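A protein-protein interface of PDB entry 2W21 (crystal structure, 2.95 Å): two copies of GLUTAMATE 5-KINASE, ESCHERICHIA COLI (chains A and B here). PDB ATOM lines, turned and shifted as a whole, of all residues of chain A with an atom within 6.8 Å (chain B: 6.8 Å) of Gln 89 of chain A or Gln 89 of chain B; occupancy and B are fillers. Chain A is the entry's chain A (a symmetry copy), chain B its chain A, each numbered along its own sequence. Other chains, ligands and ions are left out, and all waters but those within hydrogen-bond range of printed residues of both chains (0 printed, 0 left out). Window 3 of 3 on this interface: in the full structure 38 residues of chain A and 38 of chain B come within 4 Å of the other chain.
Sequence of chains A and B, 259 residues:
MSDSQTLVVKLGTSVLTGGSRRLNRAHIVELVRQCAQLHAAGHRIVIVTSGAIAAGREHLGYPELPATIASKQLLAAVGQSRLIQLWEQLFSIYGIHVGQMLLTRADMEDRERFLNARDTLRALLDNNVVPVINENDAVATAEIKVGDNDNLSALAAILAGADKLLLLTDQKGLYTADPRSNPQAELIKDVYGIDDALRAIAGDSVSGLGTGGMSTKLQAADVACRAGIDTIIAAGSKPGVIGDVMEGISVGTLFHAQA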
ATOM      1  N   ARG A  25     -25.536  -5.876   4.320  1.00  0.00           N
ATOM      2  CA  ARG A  25     -25.527  -7.158   3.622  1.00  0.00           C
ATOM      3  C   ARG A  25     -26.902  -7.841   3.531  1.00  0.00           C
ATOM      4  O   ARG A  25     -27.196  -8.483   2.550  1.00  0.00           O
ATOM      5  CB  ARG A  25     -24.469  -8.081   4.234  1.00  0.00           C
ATOM      6  CG  ARG A  25     -23.103  -7.379   4.442  1.00  0.00           C
ATOM      7  CD  ARG A  25     -21.933  -8.325   4.756  1.00  0.00           C
ATOM      8  NE  ARG A  25     -21.940  -8.737   6.162  1.00  0.00           N
ATOM      9  CZ  ARG A  25     -21.511  -9.926   6.603  1.00  0.00           C
ATOM     10  NH1 ARG A  25     -21.025 -10.831   5.736  1.00  0.00           N
ATOM     11  NH2 ARG A  25     -21.579 -10.217   7.909  1.00  0.00           N
ATOM     12  N   ARG A  82     -13.490  -3.948  -0.871  1.00  0.00           N
ATOM     13  CA  ARG A  82     -14.460  -4.602  -0.039  1.00  0.00           C
ATOM     14  C   ARG A  82     -15.762  -4.818  -0.755  1.00  0.00           C
ATOM     15  O   ARG A  82     -16.296  -5.938  -0.747  1.00  0.00           O
ATOM     16  CB  ARG A  82     -14.686  -3.750   1.169  1.00  0.00           C
ATOM     17  CG  ARG A  82     -13.469  -3.736   2.018  1.00  0.00           C
ATOM     18  CD  ARG A  82     -13.834  -4.439   3.277  1.00  0.00           C
ATOM     19  NE  ARG A  82     -12.938  -5.542   3.593  1.00  0.00           N
ATOM     20  CZ  ARG A  82     -13.315  -6.568   4.349  1.00  0.00           C
ATOM     21  NH1 ARG A  82     -14.572  -6.608   4.844  1.00  0.00           N
ATOM     22  NH2 ARG A  82     -12.434  -7.539   4.610  1.00  0.00           N
ATOM     23  N   ILE A  84     -16.287  -5.090  -3.860  1.00  0.00           N
ATOM     24  CA  ILE A  84     -16.181  -6.113  -4.888  1.00  0.00           C
ATOM     25  C   ILE A  84     -16.280  -7.509  -4.292  1.00  0.00           C
ATOM     26  O   ILE A  84     -17.142  -8.317  -4.695  1.00  0.00           O
ATOM     27  CB  ILE A  84     -14.899  -5.964  -5.768  1.00  0.00           C
ATOM     28  CG1 ILE A  84     -15.069  -6.728  -7.066  1.00  0.00           C
ATOM     29  CG2 ILE A  84     -13.648  -6.448  -5.065  1.00  0.00           C
ATOM     30  CD1 ILE A  84     -16.397  -6.522  -7.680  1.00  0.00           C
ATOM     31  N   GLN A  85     -15.390  -7.777  -3.337  1.00  0.00           N
ATOM     32  CA  GLN A  85     -15.431  -8.958  -2.466  1.00  0.00           C
ATOM     33  C   GLN A  85     -16.871  -9.248  -2.007  1.00  0.00           C
ATOM     34  O   GLN A  85     -17.396 -10.330  -2.222  1.00  0.00           O
ATOM     35  CB  GLN A  85     -14.526  -8.682  -1.280  1.00  0.00           C
ATOM     36  CG  GLN A  85     -14.402  -9.785  -0.285  1.00  0.00           C
ATOM     37  CD  GLN A  85     -13.122  -9.634   0.555  1.00  0.00           C
ATOM     38  OE1 GLN A  85     -13.106  -9.987   1.735  1.00  0.00           O
ATOM     39  NE2 GLN A  85     -12.042  -9.086  -0.057  1.00  0.00           N
ATOM     40  N   LEU A  86     -17.536  -8.256  -1.437  1.00  0.00           N
ATOM     41  CA  LEU A  86     -18.876  -8.489  -1.020  1.00  0.00           C
ATOM     42  C   LEU A  86     -19.727  -8.981  -2.166  1.00  0.00           C
ATOM     43  O   LEU A  86     -20.389  -9.971  -2.017  1.00  0.00           O
ATOM     44  CB  LEU A  86     -19.486  -7.260  -0.379  1.00  0.00           C
ATOM     45  CG  LEU A  86     -20.904  -7.561   0.089  1.00  0.00           C
ATOM     46  CD1 LEU A  86     -20.820  -8.665   1.153  1.00  0.00           C
ATOM     47  CD2 LEU A  86     -21.645  -6.356   0.637  1.00  0.00           C
ATOM     48  N   TRP A  87     -19.717  -8.315  -3.317  1.00  0.00           N
ATOM     49  CA  TRP A  87     -20.605  -8.696  -4.435  1.00  0.00           C
ATOM     50  C   TRP A  87     -20.217 -10.067  -4.975  1.00  0.00           C
ATOM     51  O   TRP A  87     -21.063 -10.846  -5.427  1.00  0.00           O
ATOM     52  CB  TRP A  87     -20.501  -7.684  -5.566  1.00  0.00           C
ATOM     53  CG  TRP A  87     -21.291  -6.445  -5.410  1.00  0.00           C
ATOM     54  CD1 TRP A  87     -20.801  -5.185  -5.129  1.00  0.00           C
ATOM     55  CD2 TRP A  87     -22.713  -6.288  -5.554  1.00  0.00           C
ATOM     56  NE1 TRP A  87     -21.832  -4.268  -5.100  1.00  0.00           N
ATOM     57  CE2 TRP A  87     -23.012  -4.919  -5.357  1.00  0.00           C
ATOM     58  CE3 TRP A  87     -23.769  -7.168  -5.829  1.00  0.00           C
ATOM     59  CZ2 TRP A  87     -24.305  -4.420  -5.433  1.00  0.00           C
ATOM     60  CZ3 TRP A  87     -25.090  -6.645  -5.913  1.00  0.00           C
ATOM     61  CH2 TRP A  87     -25.324  -5.297  -5.710  1.00  0.00           C
ATOM     62  N   GLU A  88     -18.916 -10.318  -4.945  1.00  0.00           N
ATOM     63  CA  GLU A  88     -18.342 -11.541  -5.459  1.00  0.00           C
ATOM     64  C   GLU A  88     -18.858 -12.726  -4.645  1.00  0.00           C
ATOM     65  O   GLU A  88     -19.256 -13.747  -5.227  1.00  0.00           O
ATOM     66  CB  GLU A  88     -16.802 -11.466  -5.403  1.00  0.00           C
ATOM     67  CG  GLU A  88     -16.018 -12.590  -6.107  1.00  0.00           C
ATOM     68  CD  GLU A  88     -16.286 -13.933  -5.475  1.00  0.00           C
ATOM     69  OE1 GLU A  88     -16.742 -14.866  -6.206  1.00  0.00           O
ATOM     70  OE2 GLU A  88     -16.090 -14.040  -4.230  1.00  0.00           O
ATOM     71  N   GLN A  89     -18.861 -12.581  -3.312  1.00  0.00           N
ATOM     72  CA  GLN A  89     -19.291 -13.633  -2.402  1.00  0.00           C
ATOM     73  C   GLN A  89     -20.786 -13.868  -2.406  1.00  0.00           C
ATOM     74  O   GLN A  89     -21.217 -15.014  -2.433  1.00  0.00           O
ATOM     75  CB  GLN A  89     -18.850 -13.339  -1.001  1.00  0.00           C
ATOM     76  CG  GLN A  89     -17.381 -13.620  -0.791  1.00  0.00           C
ATOM     77  CD  GLN A  89     -16.865 -12.899   0.459  1.00  0.00           C
ATOM     78  OE1 GLN A  89     -17.640 -12.202   1.145  1.00  0.00           O
ATOM     79  NE2 GLN A  89     -15.562 -13.045   0.756  1.00  0.00           N
ATOM     80  N   LEU A  90     -21.589 -12.816  -2.386  1.00  0.00           N
ATOM     81  CA  LEU A  90     -23.025 -13.032  -2.408  1.00  0.00           C
ATOM     82  C   LEU A  90     -23.471 -13.765  -3.673  1.00  0.00           C
ATOM     83  O   LEU A  90     -24.277 -14.694  -3.607  1.00  0.00           O
ATOM     84  CB  LEU A  90     -23.797 -11.741  -2.169  1.00  0.00           C
ATOM     85  CG  LEU A  90     -23.460 -11.067  -0.817  1.00  0.00           C
ATOM     86  CD1 LEU A  90     -24.347  -9.859  -0.496  1.00  0.00           C
ATOM     87  CD2 LEU A  90     -23.559 -12.038   0.335  1.00  0.00           C
ATOM     88  N   PHE A  91     -22.901 -13.404  -4.821  1.00  0.00           N
ATOM     89  CA  PHE A  91     -23.303 -14.020  -6.068  1.00  0.00           C
ATOM     90  C   PHE A  91     -22.754 -15.404  -6.114  1.00  0.00           C
ATOM     91  O   PHE A  91     -23.389 -16.359  -6.601  1.00  0.00           O
ATOM     92  CB  PHE A  91     -22.787 -13.226  -7.245  1.00  0.00           C
ATOM     93  CG  PHE A  91     -23.792 -12.259  -7.792  1.00  0.00           C
ATOM     94  CD1 PHE A  91     -23.583 -10.873  -7.693  1.00  0.00           C
ATOM     95  CD2 PHE A  91     -24.958 -12.723  -8.402  1.00  0.00           C
ATOM     96  CE1 PHE A  91     -24.524  -9.970  -8.215  1.00  0.00           C
ATOM     97  CE2 PHE A  91     -25.915 -11.822  -8.907  1.00  0.00           C
ATOM     98  CZ  PHE A  91     -25.697 -10.455  -8.823  1.00  0.00           C
ATOM     99  N   SER A  92     -21.554 -15.516  -5.577  1.00  0.00           N
ATOM    100  CA  SER A  92     -20.912 -16.819  -5.524  1.00  0.00           C
ATOM    101  C   SER A  92     -21.812 -17.856  -4.826  1.00  0.00           C
ATOM    102  O   SER A  92     -21.832 -19.017  -5.214  1.00  0.00           O
ATOM    103  CB  SER A  92     -19.549 -16.694  -4.871  1.00  0.00           C
ATOM    104  OG  SER A  92     -18.943 -17.946  -4.821  1.00  0.00           O
ATOM    105  N   ILE A  93     -22.578 -17.409  -3.828  1.00  0.00           N
ATOM    106  CA  ILE A  93     -23.531 -18.270  -3.166  1.00  0.00           C
ATOM    107  C   ILE A  93     -24.440 -18.931  -4.177  1.00  0.00           C
ATOM    108  O   ILE A  93     -24.601 -20.154  -4.140  1.00  0.00           O
ATOM    109  CB  ILE A  93     -24.360 -17.559  -2.133  1.00  0.00           C
ATOM    110  CG1 ILE A  93     -23.596 -17.475  -0.828  1.00  0.00           C
ATOM    111  CG2 ILE A  93     -25.583 -18.343  -1.832  1.00  0.00           C
ATOM    112  CD1 ILE A  93     -24.018 -16.289  -0.019  1.00  0.00           C
ATOM    113  N   TYR A  94     -25.006 -18.161  -5.104  1.00  0.00           N
ATOM    114  CA  TYR A  94     -25.862 -18.766  -6.150  1.00  0.00           C
ATOM    115  C   TYR A  94     -25.007 -19.273  -7.317  1.00  0.00           C
ATOM    116  O   TYR A  94     -25.493 -19.455  -8.433  1.00  0.00           O
ATOM    117  CB  TYR A  94     -26.938 -17.787  -6.609  1.00  0.00           C
ATOM    118  CG  TYR A  94     -27.794 -17.299  -5.463  1.00  0.00           C
ATOM    119  CD1 TYR A  94     -27.355 -16.290  -4.589  1.00  0.00           C
ATOM    120  CD2 TYR A  94     -29.048 -17.877  -5.219  1.00  0.00           C
ATOM    121  CE1 TYR A  94     -28.174 -15.869  -3.494  1.00  0.00           C
ATOM    122  CE2 TYR A  94     -29.859 -17.463  -4.144  1.00  0.00           C
ATOM    123  CZ  TYR A  94     -29.434 -16.458  -3.297  1.00  0.00           C
ATOM    124  OH  TYR A  94     -30.283 -16.085  -2.247  1.00  0.00           O
ATOM    125  N   ILE A  96     -22.986 -17.803  -9.382  1.00  0.00           N
ATOM    126  CA  ILE A  96     -22.823 -16.872 -10.492  1.00  0.00           C
ATOM    127  C   ILE A  96     -21.523 -16.109 -10.286  1.00  0.00           C
ATOM    128  O   ILE A  96     -21.282 -15.593  -9.186  1.00  0.00           O
ATOM    129  CB  ILE A  96     -23.925 -15.839 -10.437  1.00  0.00           C
ATOM    130  CG1 ILE A  96     -25.314 -16.509 -10.481  1.00  0.00           C
ATOM    131  CG2 ILE A  96     -23.692 -14.804 -11.518  1.00  0.00           C
ATOM    132  CD1 ILE A  96     -26.477 -15.582 -10.264  1.00  0.00           C
ATOM    133  N   VAL A  98     -18.672 -12.936 -11.146  1.00  0.00           N
ATOM    134  CA  VAL A  98     -18.785 -11.503 -11.323  1.00  0.00           C
ATOM    135  C   VAL A  98     -17.481 -11.025 -11.882  1.00  0.00           C
ATOM    136  O   VAL A  98     -16.461 -11.672 -11.673  1.00  0.00           O
ATOM    137  CB  VAL A  98     -19.151 -10.695 -10.023  1.00  0.00           C
ATOM    138  CG1 VAL A  98     -20.412 -11.210  -9.397  1.00  0.00           C
ATOM    139  CG2 VAL A  98     -18.000 -10.639  -9.037  1.00  0.00           C
ATOM    140  N   ARG B  25      -1.804 -19.848  -3.079  1.00  0.00           N
ATOM    141  CA  ARG B  25      -1.984 -19.162  -1.802  1.00  0.00           C
ATOM    142  C   ARG B  25      -0.890 -19.459  -0.763  1.00  0.00           C
ATOM    143  O   ARG B  25      -0.532 -18.595   0.004  1.00  0.00           O
ATOM    144  CB  ARG B  25      -3.386 -19.440  -1.252  1.00  0.00           C
ATOM    145  CG  ARG B  25      -4.499 -19.259  -2.315  1.00  0.00           C
ATOM    146  CD  ARG B  25      -5.929 -19.218  -1.753  1.00  0.00           C
ATOM    147  NE  ARG B  25      -6.425 -20.564  -1.456  1.00  0.00           N
ATOM    148  CZ  ARG B  25      -7.279 -20.853  -0.465  1.00  0.00           C
ATOM    149  NH1 ARG B  25      -7.744 -19.875   0.331  1.00  0.00           N
ATOM    150  NH2 ARG B  25      -7.657 -22.121  -0.261  1.00  0.00           N
ATOM    151  N   ARG B  82     -10.894 -11.470  -7.869  1.00  0.00           N
ATOM    152  CA  ARG B  82     -10.419 -12.537  -7.034  1.00  0.00           C
ATOM    153  C   ARG B  82      -9.086 -12.218  -6.418  1.00  0.00           C
ATOM    154  O   ARG B  82      -8.916 -12.366  -5.198  1.00  0.00           O
ATOM    155  CB  ARG B  82     -10.301 -13.767  -7.875  1.00  0.00           C
ATOM    156  CG  ARG B  82     -11.648 -14.236  -8.284  1.00  0.00           C
ATOM    157  CD  ARG B  82     -11.859 -15.540  -7.600  1.00  0.00           C
ATOM    158  NE  ARG B  82     -13.081 -15.577  -6.811  1.00  0.00           N
ATOM    159  CZ  ARG B  82     -13.234 -16.399  -5.778  1.00  0.00           C
ATOM    160  NH1 ARG B  82     -12.227 -17.230  -5.429  1.00  0.00           N
ATOM    161  NH2 ARG B  82     -14.391 -16.389  -5.108  1.00  0.00           N
ATOM    162  N   ILE B  84      -7.828  -9.387  -5.792  1.00  0.00           N
ATOM    163  CA  ILE B  84      -7.933  -8.361  -4.767  1.00  0.00           C
ATOM    164  C   ILE B  84      -8.402  -8.946  -3.444  1.00  0.00           C
ATOM    165  O   ILE B  84      -7.729  -8.796  -2.403  1.00  0.00           O
ATOM    166  CB  ILE B  84      -8.827  -7.155  -5.199  1.00  0.00           C
ATOM    167  CG1 ILE B  84      -8.531  -5.950  -4.327  1.00  0.00           C
ATOM    168  CG2 ILE B  84     -10.306  -7.468  -5.129  1.00  0.00           C
ATOM    169  CD1 ILE B  84      -7.083  -5.741  -4.116  1.00  0.00           C
ATOM    170  N   GLN B  85      -9.559  -9.607  -3.500  1.00  0.00           N
ATOM    171  CA  GLN B  85     -10.095 -10.442  -2.418  1.00  0.00           C
ATOM    172  C   GLN B  85      -8.981 -11.287  -1.776  1.00  0.00           C
ATOM    173  O   GLN B  85      -8.747 -11.220  -0.579  1.00  0.00           O
ATOM    174  CB  GLN B  85     -11.175 -11.324  -3.015  1.00  0.00           C
ATOM    175  CG  GLN B  85     -11.876 -12.232  -2.064  1.00  0.00           C
ATOM    176  CD  GLN B  85     -13.239 -12.675  -2.620  1.00  0.00           C
ATOM    177  OE1 GLN B  85     -13.678 -13.799  -2.370  1.00  0.00           O
ATOM    178  NE2 GLN B  85     -13.908 -11.787  -3.399  1.00  0.00           N
ATOM    179  N   LEU B  86      -8.245 -12.032  -2.586  1.00  0.00           N
ATOM    180  CA  LEU B  86      -7.195 -12.811  -2.024  1.00  0.00           C
ATOM    181  C   LEU B  86      -6.238 -11.948  -1.236  1.00  0.00           C
ATOM    182  O   LEU B  86      -5.953 -12.269  -0.115  1.00  0.00           O
ATOM    183  CB  LEU B  86      -6.462 -13.611  -3.080  1.00  0.00           C
ATOM    184  CG  LEU B  86      -5.374 -14.459  -2.435  1.00  0.00           C
ATOM    185  CD1 LEU B  86      -6.057 -15.444  -1.475  1.00  0.00           C
ATOM    186  CD2 LEU B  86      -4.501 -15.207  -3.426  1.00  0.00           C
ATOM    187  N   TRP B  87      -5.742 -10.848  -1.795  1.00  0.00           N
ATOM    188  CA  TRP B  87      -4.727 -10.025  -1.106  1.00  0.00           C
ATOM    189  C   TRP B  87      -5.324  -9.383   0.140  1.00  0.00           C
ATOM    190  O   TRP B  87      -4.644  -9.183   1.152  1.00  0.00           O
ATOM    191  CB  TRP B  87      -4.224  -8.921  -2.024  1.00  0.00           C
ATOM    192  CG  TRP B  87      -3.190  -9.307  -3.006  1.00  0.00           C
ATOM    193  CD1 TRP B  87      -3.359  -9.450  -4.369  1.00  0.00           C
ATOM    194  CD2 TRP B  87      -1.799  -9.575  -2.756  1.00  0.00           C
ATOM    195  NE1 TRP B  87      -2.159  -9.780  -4.967  1.00  0.00           N
ATOM    196  CE2 TRP B  87      -1.190  -9.861  -4.000  1.00  0.00           C
ATOM    197  CE3 TRP B  87      -1.004  -9.602  -1.602  1.00  0.00           C
ATOM    198  CZ2 TRP B  87       0.160 -10.161  -4.118  1.00  0.00           C
ATOM    199  CZ3 TRP B  87       0.381  -9.901  -1.734  1.00  0.00           C
ATOM    200  CH2 TRP B  87       0.924 -10.176  -2.977  1.00  0.00           C
ATOM    201  N   GLU B  88      -6.599  -9.040   0.021  1.00  0.00           N
ATOM    202  CA  GLU B  88      -7.332  -8.372   1.073  1.00  0.00           C
ATOM    203  C   GLU B  88      -7.418  -9.287   2.292  1.00  0.00           C
ATOM    204  O   GLU B  88      -7.183  -8.831   3.423  1.00  0.00           O
ATOM    205  CB  GLU B  88      -8.741  -7.989   0.573  1.00  0.00           C
ATOM    206  CG  GLU B  88      -9.586  -7.081   1.485  1.00  0.00           C
ATOM    207  CD  GLU B  88      -9.895  -7.749   2.802  1.00  0.00           C
ATOM    208  OE1 GLU B  88      -9.540  -7.168   3.874  1.00  0.00           O
ATOM    209  OE2 GLU B  88     -10.447  -8.886   2.762  1.00  0.00           O
ATOM    210  N   GLN B  89      -7.741 -10.568   2.059  1.00  0.00           N
ATOM    211  CA  GLN B  89      -7.894 -11.552   3.121  1.00  0.00           C
ATOM    212  C   GLN B  89      -6.587 -11.970   3.757  1.00  0.00           C
ATOM    213  O   GLN B  89      -6.509 -12.055   4.977  1.00  0.00           O
ATOM    214  CB  GLN B  89      -8.602 -12.773   2.618  1.00  0.00           C
ATOM    215  CG  GLN B  89     -10.088 -12.554   2.469  1.00  0.00           C
ATOM    216  CD  GLN B  89     -10.701 -13.613   1.547  1.00  0.00           C
ATOM    217  OE1 GLN B  89      -9.980 -14.498   1.042  1.00  0.00           O
ATOM    218  NE2 GLN B  89     -12.021 -13.527   1.307  1.00  0.00           N
ATOM    219  N   LEU B  90      -5.556 -12.228   2.969  1.00  0.00           N
ATOM    220  CA  LEU B  90      -4.292 -12.611   3.572  1.00  0.00           C
ATOM    221  C   LEU B  90      -3.743 -11.518   4.488  1.00  0.00           C
ATOM    222  O   LEU B  90      -3.284 -11.801   5.595  1.00  0.00           O
ATOM    223  CB  LEU B  90      -3.282 -13.074   2.529  1.00  0.00           C
ATOM    224  CG  LEU B  90      -3.772 -14.281   1.694  1.00  0.00           C
ATOM    225  CD1 LEU B  90      -2.703 -14.852   0.756  1.00  0.00           C
ATOM    226  CD2 LEU B  90      -4.274 -15.404   2.570  1.00  0.00           C
ATOM    227  N   PHE B  91      -3.848 -10.260   4.067  1.00  0.00           N
ATOM    228  CA  PHE B  91      -3.311  -9.172   4.857  1.00  0.00           C
ATOM    229  C   PHE B  91      -4.195  -8.958   6.036  1.00  0.00           C
ATOM    230  O   PHE B  91      -3.749  -8.661   7.161  1.00  0.00           O
ATOM    231  CB  PHE B  91      -3.236  -7.905   4.038  1.00  0.00           C
ATOM    232  CG  PHE B  91      -1.887  -7.676   3.426  1.00  0.00           C
ATOM    233  CD1 PHE B  91      -1.714  -7.725   2.033  1.00  0.00           C
ATOM    234  CD2 PHE B  91      -0.781  -7.417   4.235  1.00  0.00           C
ATOM    235  CE1 PHE B  91      -0.449  -7.501   1.463  1.00  0.00           C
ATOM    236  CE2 PHE B  91       0.493  -7.213   3.671  1.00  0.00           C
ATOM    237  CZ  PHE B  91       0.658  -7.245   2.294  1.00  0.00           C
ATOM    238  N   SER B  92      -5.478  -9.131   5.775  1.00  0.00           N
ATOM    239  CA  SER B  92      -6.451  -8.986   6.844  1.00  0.00           C
ATOM    240  C   SER B  92      -6.111  -9.901   8.036  1.00  0.00           C
ATOM    241  O   SER B  92      -6.315  -9.522   9.183  1.00  0.00           O
ATOM    242  CB  SER B  92      -7.847  -9.226   6.303  1.00  0.00           C
ATOM    243  OG  SER B  92      -8.773  -9.090   7.334  1.00  0.00           O
ATOM    244  N   ILE B  93      -5.555 -11.080   7.747  1.00  0.00           N
ATOM    245  CA  ILE B  93      -5.106 -11.976   8.788  1.00  0.00           C
ATOM    246  C   ILE B  93      -4.180 -11.258   9.743  1.00  0.00           C
ATOM    247  O   ILE B  93      -4.390 -11.327  10.958  1.00  0.00           O
ATOM    248  CB  ILE B  93      -4.427 -13.209   8.260  1.00  0.00           C
ATOM    249  CG1 ILE B  93      -5.463 -14.244   7.876  1.00  0.00           C
ATOM    250  CG2 ILE B  93      -3.609 -13.837   9.327  1.00  0.00           C
ATOM    251  CD1 ILE B  93      -4.961 -15.151   6.798  1.00  0.00           C
ATOM    252  N   TYR B  94      -3.187 -10.538   9.227  1.00  0.00           N
ATOM    253  CA  TYR B  94      -2.285  -9.772  10.117  1.00  0.00           C
ATOM    254  C   TYR B  94      -2.893  -8.405  10.452  1.00  0.00           C
ATOM    255  O   TYR B  94      -2.192  -7.471  10.839  1.00  0.00           O
ATOM    256  CB  TYR B  94      -0.892  -9.647   9.507  1.00  0.00           C
ATOM    257  CG  TYR B  94      -0.282 -10.994   9.193  1.00  0.00           C
ATOM    258  CD1 TYR B  94      -0.640 -11.717   8.042  1.00  0.00           C
ATOM    259  CD2 TYR B  94       0.638 -11.578  10.074  1.00  0.00           C
ATOM    260  CE1 TYR B  94      -0.069 -13.004   7.785  1.00  0.00           C
ATOM    261  CE2 TYR B  94       1.205 -12.843   9.824  1.00  0.00           C
ATOM    262  CZ  TYR B  94       0.867 -13.544   8.682  1.00  0.00           C
ATOM    263  OH  TYR B  94       1.464 -14.795   8.483  1.00  0.00           O
ATOM    264  N   ILE B  96      -3.765  -5.866   8.634  1.00  0.00           N
ATOM    265  CA  ILE B  96      -3.345  -4.765   7.776  1.00  0.00           C
ATOM    266  C   ILE B  96      -4.380  -4.601   6.672  1.00  0.00           C
ATOM    267  O   ILE B  96      -4.756  -5.593   6.032  1.00  0.00           O
ATOM    268  CB  ILE B  96      -2.054  -5.141   7.084  1.00  0.00           C
ATOM    269  CG1 ILE B  96      -0.957  -5.486   8.111  1.00  0.00           C
ATOM    270  CG2 ILE B  96      -1.678  -4.049   6.105  1.00  0.00           C
ATOM    271  CD1 ILE B  96       0.315  -6.034   7.527  1.00  0.00           C
ATOM    272  N   VAL B  98      -5.861  -2.999   2.907  1.00  0.00           N
ATOM    273  CA  VAL B  98      -5.302  -2.876   1.577  1.00  0.00           C
ATOM    274  C   VAL B  98      -6.210  -1.974   0.799  1.00  0.00           C
ATOM    275  O   VAL B  98      -7.388  -1.879   1.125  1.00  0.00           O
ATOM    276  CB  VAL B  98      -5.094  -4.234   0.810  1.00  0.00           C
ATOM    277  CG1 VAL B  98      -4.253  -5.188   1.605  1.00  0.00           C
ATOM    278  CG2 VAL B  98      -6.407  -4.853   0.369  1.00  0.00           C
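Ile 84 of chain A touches Ile 84 of chain B.
Gln 85 of chain B touches Gln 85 of chain A.
Gln 89 of chain B touches Gln 85 of chain A (NE2 to OE1, 3.7 Å).
Gln 89 of chain A touches Gln 85 of chain B (NE2 to OE1, 3.7 Å).
Gln 89 of chain A touches Gln 89 of chain B.
Of the printed residues of chain B, Arg 82 of chain A touches Glu 88 (3.0 Å).
Printed residues of chain B within 4 Å of Ile 84 of chain A: Ile 84.
Leu 86 of chain A touches none of the printed residues of chain B.
Printed residues of chain B within 4 Å of Gln 89 of chain A: Gln 85 and Gln 89.
Printed residues of chain A within 4 Å of Arg 82 of chain B: Glu 88 (3.0 Å).
Of chain A, only Gln 85 and Gln 89 come within 4 Å of Gln 89 of chain B.
The nearest residue of chain A that does not touch Gln 89 of chain B is Arg 82 of chain A (5.9 Å).
Arg 82 of chain A touches Glu 88 of chain B, and with the chains exchanged Glu 88 of chain A touches Arg 82 of chain B.
Ile 84 of chain A touches its own counterpart, Ile 84 of chain B.
Gln 85 of chain B touches its own counterpart, Gln 85 of chain A.
Gln 85 of chain A touches Glu 88 of chain B, and with the chains exchanged Glu 88 of chain A touches Gln 85 of chain B.
15 positions are printed for both chains.
Of the 9 pairs that touch across the chains among the printed residues, 9 have their exchanged pair printed and touching as well.
The side-chain amide oxygen (OE1) of Gln 85 of chain B sits close to the side-chain carboxylate (OE2) of Glu 88 of chain A (3.1 Å).
The guanidinium group of Arg 82 of chain B is in salt-bridge range of the side-chain carboxylate of Glu 88 of chain A.
OE1 of Gln 85 of chain A lies close to OE2 of Glu 88 of chain B (3.1 Å).
The guanidinium group (NH2) of Arg 82 of chain A lies within salt-bridge range of the side-chain carboxylate (OE1) of Glu 88 of chain B, at 3.0 Å.
Hydrophobic or aromatic side chains of chain B that line the printed part of chain A: Ile 84.
Hydrophobic or aromatic side chains of chain A that line the printed part of chain B: Ile 84.
Among the printed residues, 9 pairs touch across the chains.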
